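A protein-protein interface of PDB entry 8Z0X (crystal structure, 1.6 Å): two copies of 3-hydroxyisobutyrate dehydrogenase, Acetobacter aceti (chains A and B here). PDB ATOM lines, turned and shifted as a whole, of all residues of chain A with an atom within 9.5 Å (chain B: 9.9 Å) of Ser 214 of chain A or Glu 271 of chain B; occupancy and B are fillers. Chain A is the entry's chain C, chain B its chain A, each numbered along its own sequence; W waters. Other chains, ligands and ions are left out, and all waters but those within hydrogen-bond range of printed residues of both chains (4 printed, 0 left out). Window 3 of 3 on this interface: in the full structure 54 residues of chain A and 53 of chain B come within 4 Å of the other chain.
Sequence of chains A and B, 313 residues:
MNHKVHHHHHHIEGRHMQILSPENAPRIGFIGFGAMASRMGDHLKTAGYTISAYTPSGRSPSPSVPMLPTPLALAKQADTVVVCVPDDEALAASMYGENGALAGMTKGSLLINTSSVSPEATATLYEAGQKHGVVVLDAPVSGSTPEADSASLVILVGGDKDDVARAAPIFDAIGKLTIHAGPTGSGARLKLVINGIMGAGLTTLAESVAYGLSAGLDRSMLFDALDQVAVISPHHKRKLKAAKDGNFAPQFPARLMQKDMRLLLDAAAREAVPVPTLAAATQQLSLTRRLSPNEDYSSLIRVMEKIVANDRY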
ATOM      1  N   ALA A 206       2.364  21.771 -11.564  1.00  0.00           N
ATOM      2  CA  ALA A 206       1.097  22.429 -11.879  1.00  0.00           C
ATOM      3  C   ALA A 206       1.095  22.960 -13.307  1.00  0.00           C
ATOM      4  O   ALA A 206       0.096  22.835 -14.028  1.00  0.00           O
ATOM      5  CB  ALA A 206       0.822  23.557 -10.865  1.00  0.00           C
ATOM      6  N   GLU A 207       2.224  23.521 -13.755  1.00  0.00           N
ATOM      7  CA  GLU A 207       2.284  24.089 -15.097  1.00  0.00           C
ATOM      8  C   GLU A 207       2.271  23.002 -16.168  1.00  0.00           C
ATOM      9  O   GLU A 207       1.667  23.173 -17.234  1.00  0.00           O
ATOM     10  CB  GLU A 207       3.548  24.945 -15.194  1.00  0.00           C
ATOM     11  CG  GLU A 207       3.396  26.218 -14.393  1.00  0.00           C
ATOM     12  CD  GLU A 207       4.675  27.000 -14.322  1.00  0.00           C
ATOM     13  OE1 GLU A 207       5.508  26.771 -15.205  1.00  0.00           O
ATOM     14  OE2 GLU A 207       4.840  27.792 -13.366  1.00  0.00           O
ATOM     15  N   SER A 208       2.991  21.908 -15.922  1.00  0.00           N
ATOM     16  CA  SER A 208       3.038  20.817 -16.886  1.00  0.00           C
ATOM     17  C   SER A 208       1.678  20.152 -17.020  1.00  0.00           C
ATOM     18  O   SER A 208       1.235  19.864 -18.136  1.00  0.00           O
ATOM     19  CB  SER A 208       4.096  19.799 -16.474  1.00  0.00           C
ATOM     20  OG  SER A 208       5.374  20.432 -16.358  1.00  0.00           O
ATOM     21  N   VAL A 209       1.008  19.903 -15.886  1.00  0.00           N
ATOM     22  CA  VAL A 209      -0.365  19.404 -15.929  1.00  0.00           C
ATOM     23  C   VAL A 209      -1.264  20.362 -16.698  1.00  0.00           C
ATOM     24  O   VAL A 209      -2.054  19.946 -17.550  1.00  0.00           O
ATOM     25  CB  VAL A 209      -0.883  19.170 -14.502  1.00  0.00           C
ATOM     26  CG1 VAL A 209      -2.393  18.952 -14.506  1.00  0.00           C
ATOM     27  CG2 VAL A 209      -0.170  17.971 -13.887  1.00  0.00           C
ATOM     28  N   ALA A 210      -1.126  21.664 -16.444  1.00  0.00           N
ATOM     29  CA  ALA A 210      -1.958  22.637 -17.143  1.00  0.00           C
ATOM     30  C   ALA A 210      -1.746  22.579 -18.649  1.00  0.00           C
ATOM     31  O   ALA A 210      -2.719  22.636 -19.414  1.00  0.00           O
ATOM     32  CB  ALA A 210      -1.678  24.040 -16.612  1.00  0.00           C
ATOM     33  N   TYR A 211      -0.484  22.481 -19.104  1.00  0.00           N
ATOM     34  CA  TYR A 211      -0.260  22.345 -20.540  1.00  0.00           C
ATOM     35  C   TYR A 211      -0.971  21.098 -21.061  1.00  0.00           C
ATOM     36  O   TYR A 211      -1.696  21.158 -22.056  1.00  0.00           O
ATOM     37  CB  TYR A 211       1.248  22.318 -20.904  1.00  0.00           C
ATOM     38  CG  TYR A 211       1.344  21.783 -22.308  1.00  0.00           C
ATOM     39  CD1 TYR A 211       0.898  22.549 -23.399  1.00  0.00           C
ATOM     40  CD2 TYR A 211       1.734  20.465 -22.546  1.00  0.00           C
ATOM     41  CE1 TYR A 211       0.885  22.025 -24.686  1.00  0.00           C
ATOM     42  CE2 TYR A 211       1.713  19.940 -23.823  1.00  0.00           C
ATOM     43  CZ  TYR A 211       1.291  20.721 -24.883  1.00  0.00           C
ATOM     44  OH  TYR A 211       1.246  20.183 -26.145  1.00  0.00           O
ATOM     45  N   GLY A 212      -0.797  19.964 -20.374  1.00  0.00           N
ATOM     46  CA  GLY A 212      -1.403  18.732 -20.856  1.00  0.00           C
ATOM     47  C   GLY A 212      -2.910  18.853 -21.003  1.00  0.00           C
ATOM     48  O   GLY A 212      -3.488  18.402 -22.000  1.00  0.00           O
ATOM     49  N   LEU A 213      -3.563  19.454 -20.004  1.00  0.00           N
ATOM     50  CA  LEU A 213      -5.011  19.628 -20.084  1.00  0.00           C
ATOM     51  C   LEU A 213      -5.393  20.564 -21.225  1.00  0.00           C
ATOM     52  O   LEU A 213      -6.366  20.313 -21.959  1.00  0.00           O
ATOM     53  CB  LEU A 213      -5.537  20.149 -18.751  1.00  0.00           C
ATOM     54  CG  LEU A 213      -5.378  19.158 -17.607  1.00  0.00           C
ATOM     55  CD1 LEU A 213      -5.704  19.846 -16.285  1.00  0.00           C
ATOM     56  CD2 LEU A 213      -6.286  17.945 -17.825  1.00  0.00           C
ATOM     57  N   SER A 214      -4.632  21.649 -21.401  1.00  0.00           N
ATOM     58  CA  SER A 214      -4.928  22.599 -22.467  1.00  0.00           C
ATOM     59  C   SER A 214      -4.786  21.975 -23.845  1.00  0.00           C
ATOM     60  O   SER A 214      -5.442  22.419 -24.798  1.00  0.00           O
ATOM     61  CB  SER A 214      -4.008  23.809 -22.354  1.00  0.00           C
ATOM     62  OG  SER A 214      -2.708  23.541 -22.892  1.00  0.00           O
ATOM     63  N   ALA A 215      -3.939  20.957 -23.964  1.00  0.00           N
ATOM     64  CA  ALA A 215      -3.669  20.267 -25.209  1.00  0.00           C
ATOM     65  C   ALA A 215      -4.630  19.116 -25.449  1.00  0.00           C
ATOM     66  O   ALA A 215      -4.437  18.343 -26.396  1.00  0.00           O
ATOM     67  CB  ALA A 215      -2.213  19.784 -25.216  1.00  0.00           C
ATOM     68  N   GLY A 216      -5.643  18.980 -24.602  1.00  0.00           N
ATOM     69  CA  GLY A 216      -6.720  18.035 -24.820  1.00  0.00           C
ATOM     70  C   GLY A 216      -6.573  16.696 -24.129  1.00  0.00           C
ATOM     71  O   GLY A 216      -7.432  15.823 -24.326  1.00  0.00           O
ATOM     72  N   LEU A 217      -5.535  16.502 -23.316  1.00  0.00           N
ATOM     73  CA  LEU A 217      -5.351  15.208 -22.669  1.00  0.00           C
ATOM     74  C   LEU A 217      -6.432  14.957 -21.628  1.00  0.00           C
ATOM     75  O   LEU A 217      -6.806  15.852 -20.862  1.00  0.00           O
ATOM     76  CB  LEU A 217      -3.984  15.135 -21.990  1.00  0.00           C
ATOM     77  CG  LEU A 217      -2.788  15.110 -22.935  1.00  0.00           C
ATOM     78  CD1 LEU A 217      -1.514  15.013 -22.114  1.00  0.00           C
ATOM     79  CD2 LEU A 217      -2.897  13.952 -23.923  1.00  0.00           C
ATOM     80  N   ASP A 218      -6.909  13.712 -21.585  1.00  0.00           N
ATOM     81  CA  ASP A 218      -7.881  13.320 -20.572  1.00  0.00           C
ATOM     82  C   ASP A 218      -7.293  13.496 -19.176  1.00  0.00           C
ATOM     83  O   ASP A 218      -6.166  13.063 -18.908  1.00  0.00           O
ATOM     84  CB  ASP A 218      -8.292  11.858 -20.798  1.00  0.00           C
ATOM     85  CG  ASP A 218      -9.246  11.349 -19.733  1.00  0.00           C
ATOM     86  OD1 ASP A 218     -10.446  11.644 -19.844  1.00  0.00           O
ATOM     87  OD2 ASP A 218      -8.807  10.679 -18.784  1.00  0.00           O
ATOM     88  N   ARG A 219      -8.068  14.107 -18.269  1.00  0.00           N
ATOM     89  CA  ARG A 219      -7.532  14.478 -16.963  1.00  0.00           C
ATOM     90  C   ARG A 219      -7.144  13.257 -16.127  1.00  0.00           C
ATOM     91  O   ARG A 219      -6.057  13.215 -15.555  1.00  0.00           O
ATOM     92  CB  ARG A 219      -8.539  15.352 -16.208  1.00  0.00           C
ATOM     93  CG  ARG A 219      -8.044  15.820 -14.861  1.00  0.00           C
ATOM     94  CD  ARG A 219      -9.108  16.682 -14.167  1.00  0.00           C
ATOM     95  NE  ARG A 219      -8.623  17.317 -12.946  1.00  0.00           N
ATOM     96  CZ  ARG A 219      -8.557  16.728 -11.759  1.00  0.00           C
ATOM     97  NH1 ARG A 219      -8.910  15.459 -11.596  1.00  0.00           N
ATOM     98  NH2 ARG A 219      -8.134  17.430 -10.712  1.00  0.00           N
ATOM     99  N   LEU A 222      -4.078  11.608 -17.439  1.00  0.00           N
ATOM    100  CA  LEU A 222      -2.882  12.425 -17.221  1.00  0.00           C
ATOM    101  C   LEU A 222      -2.382  12.312 -15.785  1.00  0.00           C
ATOM    102  O   LEU A 222      -1.198  12.059 -15.544  1.00  0.00           O
ATOM    103  CB  LEU A 222      -3.198  13.872 -17.603  1.00  0.00           C
ATOM    104  CG  LEU A 222      -2.115  14.907 -17.306  1.00  0.00           C
ATOM    105  CD1 LEU A 222      -0.804  14.558 -18.045  1.00  0.00           C
ATOM    106  CD2 LEU A 222      -2.645  16.281 -17.699  1.00  0.00           C
ATOM    107  N   MET A 304      -4.194  26.490 -11.756  1.00  0.00           N
ATOM    108  CA  MET A 304      -3.835  26.349 -13.163  1.00  0.00           C
ATOM    109  C   MET A 304      -4.907  25.627 -13.960  1.00  0.00           C
ATOM    110  O   MET A 304      -5.171  26.003 -15.103  1.00  0.00           O
ATOM    111  CB  MET A 304      -2.489  25.633 -13.291  1.00  0.00           C
ATOM    112  CG  MET A 304      -1.225  26.336 -12.791  1.00  0.00           C
ATOM    113  SD  MET A 304      -1.020  27.983 -13.494  1.00  0.00           S
ATOM    114  CE  MET A 304      -0.687  27.476 -15.172  1.00  0.00           C
ATOM    115  N   GLU A 305      -5.508  24.570 -13.402  1.00  0.00           N
ATOM    116  CA  GLU A 305      -6.636  23.925 -14.084  1.00  0.00           C
ATOM    117  C   GLU A 305      -7.738  24.929 -14.406  1.00  0.00           C
ATOM    118  O   GLU A 305      -8.327  24.885 -15.497  1.00  0.00           O
ATOM    119  CB  GLU A 305      -7.211  22.801 -13.220  1.00  0.00           C
ATOM    120  CG  GLU A 305      -6.293  21.603 -13.004  1.00  0.00           C
ATOM    121  CD  GLU A 305      -7.086  20.445 -12.419  1.00  0.00           C
ATOM    122  OE1 GLU A 305      -6.653  19.905 -11.383  1.00  0.00           O
ATOM    123  OE2 GLU A 305      -8.123  20.069 -13.013  1.00  0.00           O
ATOM    124  N   ILE A 307      -7.428  28.206 -14.808  1.00  0.00           N
ATOM    125  CA  ILE A 307      -6.985  29.078 -15.899  1.00  0.00           C
ATOM    126  C   ILE A 307      -7.234  28.407 -17.243  1.00  0.00           C
ATOM    127  O   ILE A 307      -7.734  29.039 -18.187  1.00  0.00           O
ATOM    128  CB  ILE A 307      -5.503  29.462 -15.727  1.00  0.00           C
ATOM    129  CG1 ILE A 307      -5.332  30.399 -14.535  1.00  0.00           C
ATOM    130  CG2 ILE A 307      -4.966  30.110 -17.031  1.00  0.00           C
ATOM    131  CD1 ILE A 307      -3.867  30.653 -14.151  1.00  0.00           C
ATOM    132  N   VAL A 308      -6.909  27.116 -17.345  1.00  0.00           N
ATOM    133  CA  VAL A 308      -7.029  26.399 -18.608  1.00  0.00           C
ATOM    134  C   VAL A 308      -8.492  26.162 -18.961  1.00  0.00           C
ATOM    135  O   VAL A 308      -8.882  26.217 -20.131  1.00  0.00           O
ATOM    136  CB  VAL A 308      -6.235  25.079 -18.531  1.00  0.00           C
ATOM    137  CG1 VAL A 308      -6.656  24.102 -19.637  1.00  0.00           C
ATOM    138  CG2 VAL A 308      -4.729  25.380 -18.591  1.00  0.00           C
ATOM    139  N   ALA A 309      -9.328  25.911 -17.960  1.00  0.00           N
ATOM    140  CA  ALA A 309     -10.743  25.707 -18.227  1.00  0.00           C
ATOM    141  C   ALA A 309     -11.486  27.001 -18.506  1.00  0.00           C
ATOM    142  O   ALA A 309     -12.678  26.941 -18.833  1.00  0.00           O
ATOM    143  CB  ALA A 309     -11.405  25.010 -17.037  1.00  0.00           C
ATOM    144  N   ASN A 310     -10.829  28.154 -18.367  1.00  0.00           N
ATOM    145  CA  ASN A 310     -11.520  29.438 -18.344  1.00  0.00           C
ATOM    146  C   ASN A 310     -12.616  29.405 -17.283  1.00  0.00           C
ATOM    147  O   ASN A 310     -13.771  29.762 -17.525  1.00  0.00           O
ATOM    148  CB  ASN A 310     -12.056  29.801 -19.734  1.00  0.00           C
ATOM    149  CG  ASN A 310     -10.993  29.674 -20.822  1.00  0.00           C
ATOM    150  OD1 ASN A 310      -9.826  29.998 -20.600  1.00  0.00           O
ATOM    151  ND2 ASN A 310     -11.386  29.180 -21.991  1.00  0.00           N
ATOM    152  N   PRO B 119       3.763  18.521 -31.629  1.00  0.00           N
ATOM    153  CA  PRO B 119       2.406  18.087 -31.999  1.00  0.00           C
ATOM    154  C   PRO B 119       2.092  18.323 -33.461  1.00  0.00           C
ATOM    155  O   PRO B 119       1.346  17.536 -34.062  1.00  0.00           O
ATOM    156  CB  PRO B 119       1.505  18.937 -31.090  1.00  0.00           C
ATOM    157  CG  PRO B 119       2.384  19.249 -29.901  1.00  0.00           C
ATOM    158  CD  PRO B 119       3.748  19.458 -30.486  1.00  0.00           C
ATOM    159  N   GLU B 120       2.656  19.374 -34.055  1.00  0.00           N
ATOM    160  CA  GLU B 120       2.426  19.642 -35.474  1.00  0.00           C
ATOM    161  C   GLU B 120       3.066  18.568 -36.345  1.00  0.00           C
ATOM    162  O   GLU B 120       2.439  18.067 -37.286  1.00  0.00           O
ATOM    163  CB  GLU B 120       2.965  21.029 -35.836  1.00  0.00           C
ATOM    164  CG  GLU B 120       2.162  22.203 -35.271  1.00  0.00           C
ATOM    165  CD  GLU B 120       2.238  22.313 -33.753  1.00  0.00           C
ATOM    166  OE1 GLU B 120       3.357  22.269 -33.214  1.00  0.00           O
ATOM    167  OE2 GLU B 120       1.176  22.477 -33.106  1.00  0.00           O
ATOM    168  N   GLY B 185      -1.724  11.966 -31.474  1.00  0.00           N
ATOM    169  CA  GLY B 185      -1.238  13.208 -30.917  1.00  0.00           C
ATOM    170  C   GLY B 185      -1.157  13.225 -29.407  1.00  0.00           C
ATOM    171  O   GLY B 185      -0.447  14.078 -28.845  1.00  0.00           O
ATOM    172  N   ARG B 189       1.914  14.734 -26.858  1.00  0.00           N
ATOM    173  CA  ARG B 189       1.611  15.753 -25.850  1.00  0.00           C
ATOM    174  C   ARG B 189       2.002  15.305 -24.451  1.00  0.00           C
ATOM    175  O   ARG B 189       2.534  16.101 -23.669  1.00  0.00           O
ATOM    176  CB  ARG B 189       0.124  16.116 -25.890  1.00  0.00           C
ATOM    177  CG  ARG B 189      -0.262  16.913 -27.128  1.00  0.00           C
ATOM    178  CD  ARG B 189      -1.743  16.755 -27.412  1.00  0.00           C
ATOM    179  NE  ARG B 189      -2.218  17.702 -28.410  1.00  0.00           N
ATOM    180  CZ  ARG B 189      -1.962  17.603 -29.703  1.00  0.00           C
ATOM    181  NH1 ARG B 189      -1.232  16.613 -30.186  1.00  0.00           N
ATOM    182  NH2 ARG B 189      -2.440  18.526 -30.533  1.00  0.00           N
ATOM    183  N   LEU B 192       5.658  15.757 -24.014  1.00  0.00           N
ATOM    184  CA  LEU B 192       5.988  17.157 -23.726  1.00  0.00           C
ATOM    185  C   LEU B 192       5.797  17.471 -22.248  1.00  0.00           C
ATOM    186  O   LEU B 192       6.652  18.123 -21.622  1.00  0.00           O
ATOM    187  CB  LEU B 192       5.127  18.105 -24.576  1.00  0.00           C
ATOM    188  CG  LEU B 192       5.744  18.622 -25.881  1.00  0.00           C
ATOM    189  CD1 LEU B 192       6.081  17.467 -26.767  1.00  0.00           C
ATOM    190  CD2 LEU B 192       4.788  19.594 -26.594  1.00  0.00           C
ATOM    191  N   VAL B 193       4.672  17.020 -21.670  1.00  0.00           N
ATOM    192  CA  VAL B 193       4.403  17.208 -20.240  1.00  0.00           C
ATOM    193  C   VAL B 193       5.549  16.661 -19.407  1.00  0.00           C
ATOM    194  O   VAL B 193       6.078  17.338 -18.512  1.00  0.00           O
ATOM    195  CB  VAL B 193       3.072  16.539 -19.850  1.00  0.00           C
ATOM    196  CG1 VAL B 193       2.922  16.522 -18.344  1.00  0.00           C
ATOM    197  CG2 VAL B 193       1.892  17.253 -20.503  1.00  0.00           C
ATOM    198  N   LEU B 263      10.228  22.854 -27.790  1.00  0.00           N
ATOM    199  CA  LEU B 263       8.970  22.338 -28.325  1.00  0.00           C
ATOM    200  C   LEU B 263       7.834  22.528 -27.335  1.00  0.00           C
ATOM    201  O   LEU B 263       6.719  22.920 -27.718  1.00  0.00           O
ATOM    202  CB  LEU B 263       9.112  20.853 -28.652  1.00  0.00           C
ATOM    203  CG  LEU B 263      10.137  20.457 -29.717  1.00  0.00           C
ATOM    204  CD1 LEU B 263       9.968  18.965 -29.988  1.00  0.00           C
ATOM    205  CD2 LEU B 263       9.977  21.276 -30.978  1.00  0.00           C
ATOM    206  N   LEU B 264       8.092  22.238 -26.056  1.00  0.00           N
ATOM    207  CA  LEU B 264       7.068  22.401 -25.033  1.00  0.00           C
ATOM    208  C   LEU B 264       6.640  23.848 -24.912  1.00  0.00           C
ATOM    209  O   LEU B 264       5.440  24.138 -24.819  1.00  0.00           O
ATOM    210  CB  LEU B 264       7.601  21.891 -23.697  1.00  0.00           C
ATOM    211  CG  LEU B 264       6.761  22.214 -22.469  1.00  0.00           C
ATOM    212  CD1 LEU B 264       5.374  21.613 -22.528  1.00  0.00           C
ATOM    213  CD2 LEU B 264       7.514  21.700 -21.255  1.00  0.00           C
ATOM    214  N   LEU B 265       7.601  24.774 -24.906  1.00  0.00           N
ATOM    215  CA  LEU B 265       7.223  26.169 -24.718  1.00  0.00           C
ATOM    216  C   LEU B 265       6.520  26.711 -25.958  1.00  0.00           C
ATOM    217  O   LEU B 265       5.613  27.544 -25.827  1.00  0.00           O
ATOM    218  CB  LEU B 265       8.457  26.998 -24.332  1.00  0.00           C
ATOM    219  CG  LEU B 265       8.720  26.984 -22.808  1.00  0.00           C
ATOM    220  CD1 LEU B 265       7.772  27.906 -22.087  1.00  0.00           C
ATOM    221  CD2 LEU B 265       8.652  25.584 -22.152  1.00  0.00           C
ATOM    222  N   ASP B 266       6.865  26.208 -27.158  1.00  0.00           N
ATOM    223  CA  ASP B 266       6.106  26.593 -28.340  1.00  0.00           C
ATOM    224  C   ASP B 266       4.673  26.112 -28.220  1.00  0.00           C
ATOM    225  O   ASP B 266       3.731  26.855 -28.509  1.00  0.00           O
ATOM    226  CB  ASP B 266       6.741  26.007 -29.604  1.00  0.00           C
ATOM    227  CG  ASP B 266       6.036  26.476 -30.839  1.00  0.00           C
ATOM    228  OD1 ASP B 266       6.301  27.626 -31.239  1.00  0.00           O
ATOM    229  OD2 ASP B 266       5.138  25.753 -31.330  1.00  0.00           O
ATOM    230  N   ALA B 267       4.495  24.865 -27.784  1.00  0.00           N
ATOM    231  CA  ALA B 267       3.143  24.316 -27.687  1.00  0.00           C
ATOM    232  C   ALA B 267       2.338  25.035 -26.619  1.00  0.00           C
ATOM    233  O   ALA B 267       1.152  25.337 -26.818  1.00  0.00           O
ATOM    234  CB  ALA B 267       3.220  22.816 -27.388  1.00  0.00           C
ATOM    235  N   ALA B 268       2.967  25.323 -25.477  1.00  0.00           N
ATOM    236  CA  ALA B 268       2.270  26.042 -24.421  1.00  0.00           C
ATOM    237  C   ALA B 268       1.866  27.431 -24.888  1.00  0.00           C
ATOM    238  O   ALA B 268       0.797  27.924 -24.507  1.00  0.00           O
ATOM    239  CB  ALA B 268       3.148  26.134 -23.167  1.00  0.00           C
ATOM    240  N   ALA B 269       2.696  28.071 -25.726  1.00  0.00           N
ATOM    241  CA  ALA B 269       2.335  29.382 -26.267  1.00  0.00           C
ATOM    242  C   ALA B 269       1.174  29.259 -27.252  1.00  0.00           C
ATOM    243  O   ALA B 269       0.245  30.077 -27.229  1.00  0.00           O
ATOM    244  CB  ALA B 269       3.547  30.049 -26.937  1.00  0.00           C
ATOM    245  N   ARG B 270       1.191  28.230 -28.112  1.00  0.00           N
ATOM    246  CA  ARG B 270       0.064  28.037 -29.021  1.00  0.00           C
ATOM    247  C   ARG B 270      -1.230  27.793 -28.262  1.00  0.00           C
ATOM    248  O   ARG B 270      -2.302  28.229 -28.712  1.00  0.00           O
ATOM    249  CB  ARG B 270       0.346  26.884 -29.979  1.00  0.00           C
ATOM    250  CG  ARG B 270       1.342  27.262 -31.067  1.00  0.00           C
ATOM    251  CD  ARG B 270       1.668  26.077 -31.935  1.00  0.00           C
ATOM    252  NE  ARG B 270       2.648  26.388 -32.967  1.00  0.00           N
ATOM    253  CZ  ARG B 270       2.352  26.925 -34.143  1.00  0.00           C
ATOM    254  NH1 ARG B 270       1.111  27.258 -34.460  1.00  0.00           N
ATOM    255  NH2 ARG B 270       3.323  27.114 -35.032  1.00  0.00           N
ATOM    256  N   GLU B 271      -1.157  27.124 -27.107  1.00  0.00           N
ATOM    257  CA  GLU B 271      -2.343  26.875 -26.289  1.00  0.00           C
ATOM    258  C   GLU B 271      -2.668  28.044 -25.361  1.00  0.00           C
ATOM    259  O   GLU B 271      -3.656  27.973 -24.620  1.00  0.00           O
ATOM    260  CB  GLU B 271      -2.150  25.625 -25.421  1.00  0.00           C
ATOM    261  CG  GLU B 271      -1.969  24.228 -26.082  1.00  0.00           C
ATOM    262  CD  GLU B 271      -2.968  23.840 -27.150  1.00  0.00           C
ATOM    263  OE1 GLU B 271      -4.102  24.367 -27.161  1.00  0.00           O
ATOM    264  OE2 GLU B 271      -2.664  22.883 -27.903  1.00  0.00           O
ATOM    265  N   ALA B 272      -1.840  29.091 -25.356  1.00  0.00           N
ATOM    266  CA  ALA B 272      -1.997  30.250 -24.473  1.00  0.00           C
ATOM    267  C   ALA B 272      -2.121  29.839 -23.009  1.00  0.00           C
ATOM    268  O   ALA B 272      -3.003  30.297 -22.273  1.00  0.00           O
ATOM    269  CB  ALA B 272      -3.190  31.118 -24.900  1.00  0.00           C
ATOM    270  N   VAL B 273      -1.188  29.007 -22.553  1.00  0.00           N
ATOM    271  CA  VAL B 273      -1.128  28.576 -21.162  1.00  0.00           C
ATOM    272  C   VAL B 273       0.118  29.181 -20.533  1.00  0.00           C
ATOM    273  O   VAL B 273       1.230  28.917 -21.015  1.00  0.00           O
ATOM    274  CB  VAL B 273      -1.099  27.048 -21.045  1.00  0.00           C
ATOM    275  CG1 VAL B 273      -1.120  26.613 -19.569  1.00  0.00           C
ATOM    276  CG2 VAL B 273      -2.255  26.511 -21.784  1.00  0.00           C
ATOM    277  N   PRO B 274      -0.013  30.004 -19.499  1.00  0.00           N
ATOM    278  CA  PRO B 274       1.180  30.612 -18.874  1.00  0.00           C
ATOM    279  C   PRO B 274       1.952  29.593 -18.050  1.00  0.00           C
ATOM    280  O   PRO B 274       1.427  29.034 -17.080  1.00  0.00           O
ATOM    281  CB  PRO B 274       0.603  31.728 -17.996  1.00  0.00           C
ATOM    282  CG  PRO B 274      -0.857  31.345 -17.739  1.00  0.00           C
ATOM    283  CD  PRO B 274      -1.287  30.455 -18.888  1.00  0.00           C
ATOM    284  N   VAL B 275       3.218  29.392 -18.406  1.00  0.00           N
ATOM    285  CA  VAL B 275       4.055  28.401 -17.727  1.00  0.00           C
ATOM    286  C   VAL B 275       5.388  29.053 -17.348  1.00  0.00           C
ATOM    287  O   VAL B 275       6.445  28.685 -17.887  1.00  0.00           O
ATOM    288  CB  VAL B 275       4.212  27.125 -18.577  1.00  0.00           C
ATOM    289  CG1 VAL B 275       2.824  26.401 -18.668  1.00  0.00           C
ATOM    290  CG2 VAL B 275       4.771  27.371 -19.983  1.00  0.00           C
ATOM    291  N   LEU B 278       8.403  26.636 -16.227  1.00  0.00           N
ATOM    292  CA  LEU B 278       8.938  25.918 -17.382  1.00  0.00           C
ATOM    293  C   LEU B 278       9.688  26.860 -18.307  1.00  0.00           C
ATOM    294  O   LEU B 278      10.695  26.477 -18.910  1.00  0.00           O
ATOM    295  CB  LEU B 278       7.802  25.219 -18.143  1.00  0.00           C
ATOM    296  CG  LEU B 278       6.958  24.241 -17.317  1.00  0.00           C
ATOM    297  CD1 LEU B 278       5.852  23.654 -18.162  1.00  0.00           C
ATOM    298  CD2 LEU B 278       7.843  23.144 -16.772  1.00  0.00           C
HETATM  299  O   HOH W   1      -5.789  25.653 -25.439  1.00  0.00           O
HETATM  300  O   HOH W   2       0.695  30.947 -14.384  1.00  0.00           O
HETATM  301  O   HOH W   3      -3.827  20.477 -28.788  1.00  0.00           O
HETATM  302  O   HOH W   4      -0.258  21.542 -28.013  1.00  0.00           O
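NE of Arg 189 of chain B lies within hydrogen-bond range of O of Ala 215 of chain A, at 3.1 Å. The backbone NH (N) of Leu 278 of chain B sits at hydrogen-bond distance from the side-chain carboxylate (OE1) of Glu 207 of chain A (3.1 Å). The side-chain carboxylate (OE1) of Glu 207 of chain A sits close to the backbone carbonyl oxygen (O) of Val 275 of chain B. The backbone carbonyl oxygen of Ser 214 of chain A lies close to the side-chain carboxylate of Glu 271 of chain B (3.3 Å).
O of Gly 185 of chain B sits at hydrogen-bond distance from NH1 of Arg 189 of chain B, 3.0 Å away. The backbone NH of Val 273 of chain B sits at hydrogen-bond distance from the backbone carbonyl oxygen of Ala 268 of chain B, 3.0 Å away. O of Tyr 211 of chain A lies within hydrogen-bond range of OG of Ser 214 of chain A (2.7 Å).
Ser 208 of chain A touches Val 193 of chain B (O to CG2, 3.6 Å). Val 193 of chain B touches Tyr 211 of chain A. Tyr 211 of chain A touches Glu 271 of chain B. Gly 212 of chain A touches Val 193 of chain B. Ser 214 of chain A touches Val 273 of chain B. Ala 215 of chain A touches Glu 271 of chain B (CA to OE2, 3.9 Å).
Tyr 211 of chain A touches just these residues of chain B: Arg 189, Leu 192, Val 193, Leu 264, Ala 267, Ala 268 and Glu 271. Gly 212 of chain A touches just one residue of chain B: Val 193 (3.6 Å). Of the printed residues of chain B, Val 308 of chain A touches Val 273 (3.9 Å). Of the printed residues of chain A, Leu 264 of chain B touches Tyr 211. Of the printed residues of chain A, Ala 267 of chain B touches Tyr 211 (3.5 Å). Printed residues of chain A within 4 Å of Ala 268 of chain B: Tyr 211 (3.9 Å). Glu 271 of chain B touches three residues of chain A. No residue of chain A comes within 4 Å of Ala 272 of chain B. The nearest residue of chain A that does not touch Glu 271 of chain B is Gly 216 of chain A (5.9 Å).
Of the 20 printed residues of chain B, 11 touch a printed residue of chain A. Hydrophobic or aromatic side chains of chain B within 4 Å of the printed part of chain A: Leu 192, Val 193, Leu 264, Ala 267, Val 273, Val 275 and Leu 278. Of the 21 printed residues of chain A, 9 touch a printed residue of chain B. Printed residues of chain A that touch a printed residue of chain B: Glu 207, Ser 208, Ala 210, Tyr 211, Gly 212, Ser 214, Ala 215, Met 304 and Val 308. Hydrophobic or aromatic side chains of chain A within 4 Å of the printed part of chain B: Ala 210, Tyr 211, Ala 215, Met 304 and Val 308. Among the printed residues, no Asp or Glu carboxylate lies within 4 Å of a Lys or Arg side-chain nitrogen of the other chain.
No position is printed for both chains.
Water W2 lies within hydrogen-bond range of the backbone carbonyl oxygen of Pro 274 of chain B (3.4 Å) and the side-chain sulfur of Met 304 of chain A (3.5 Å).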
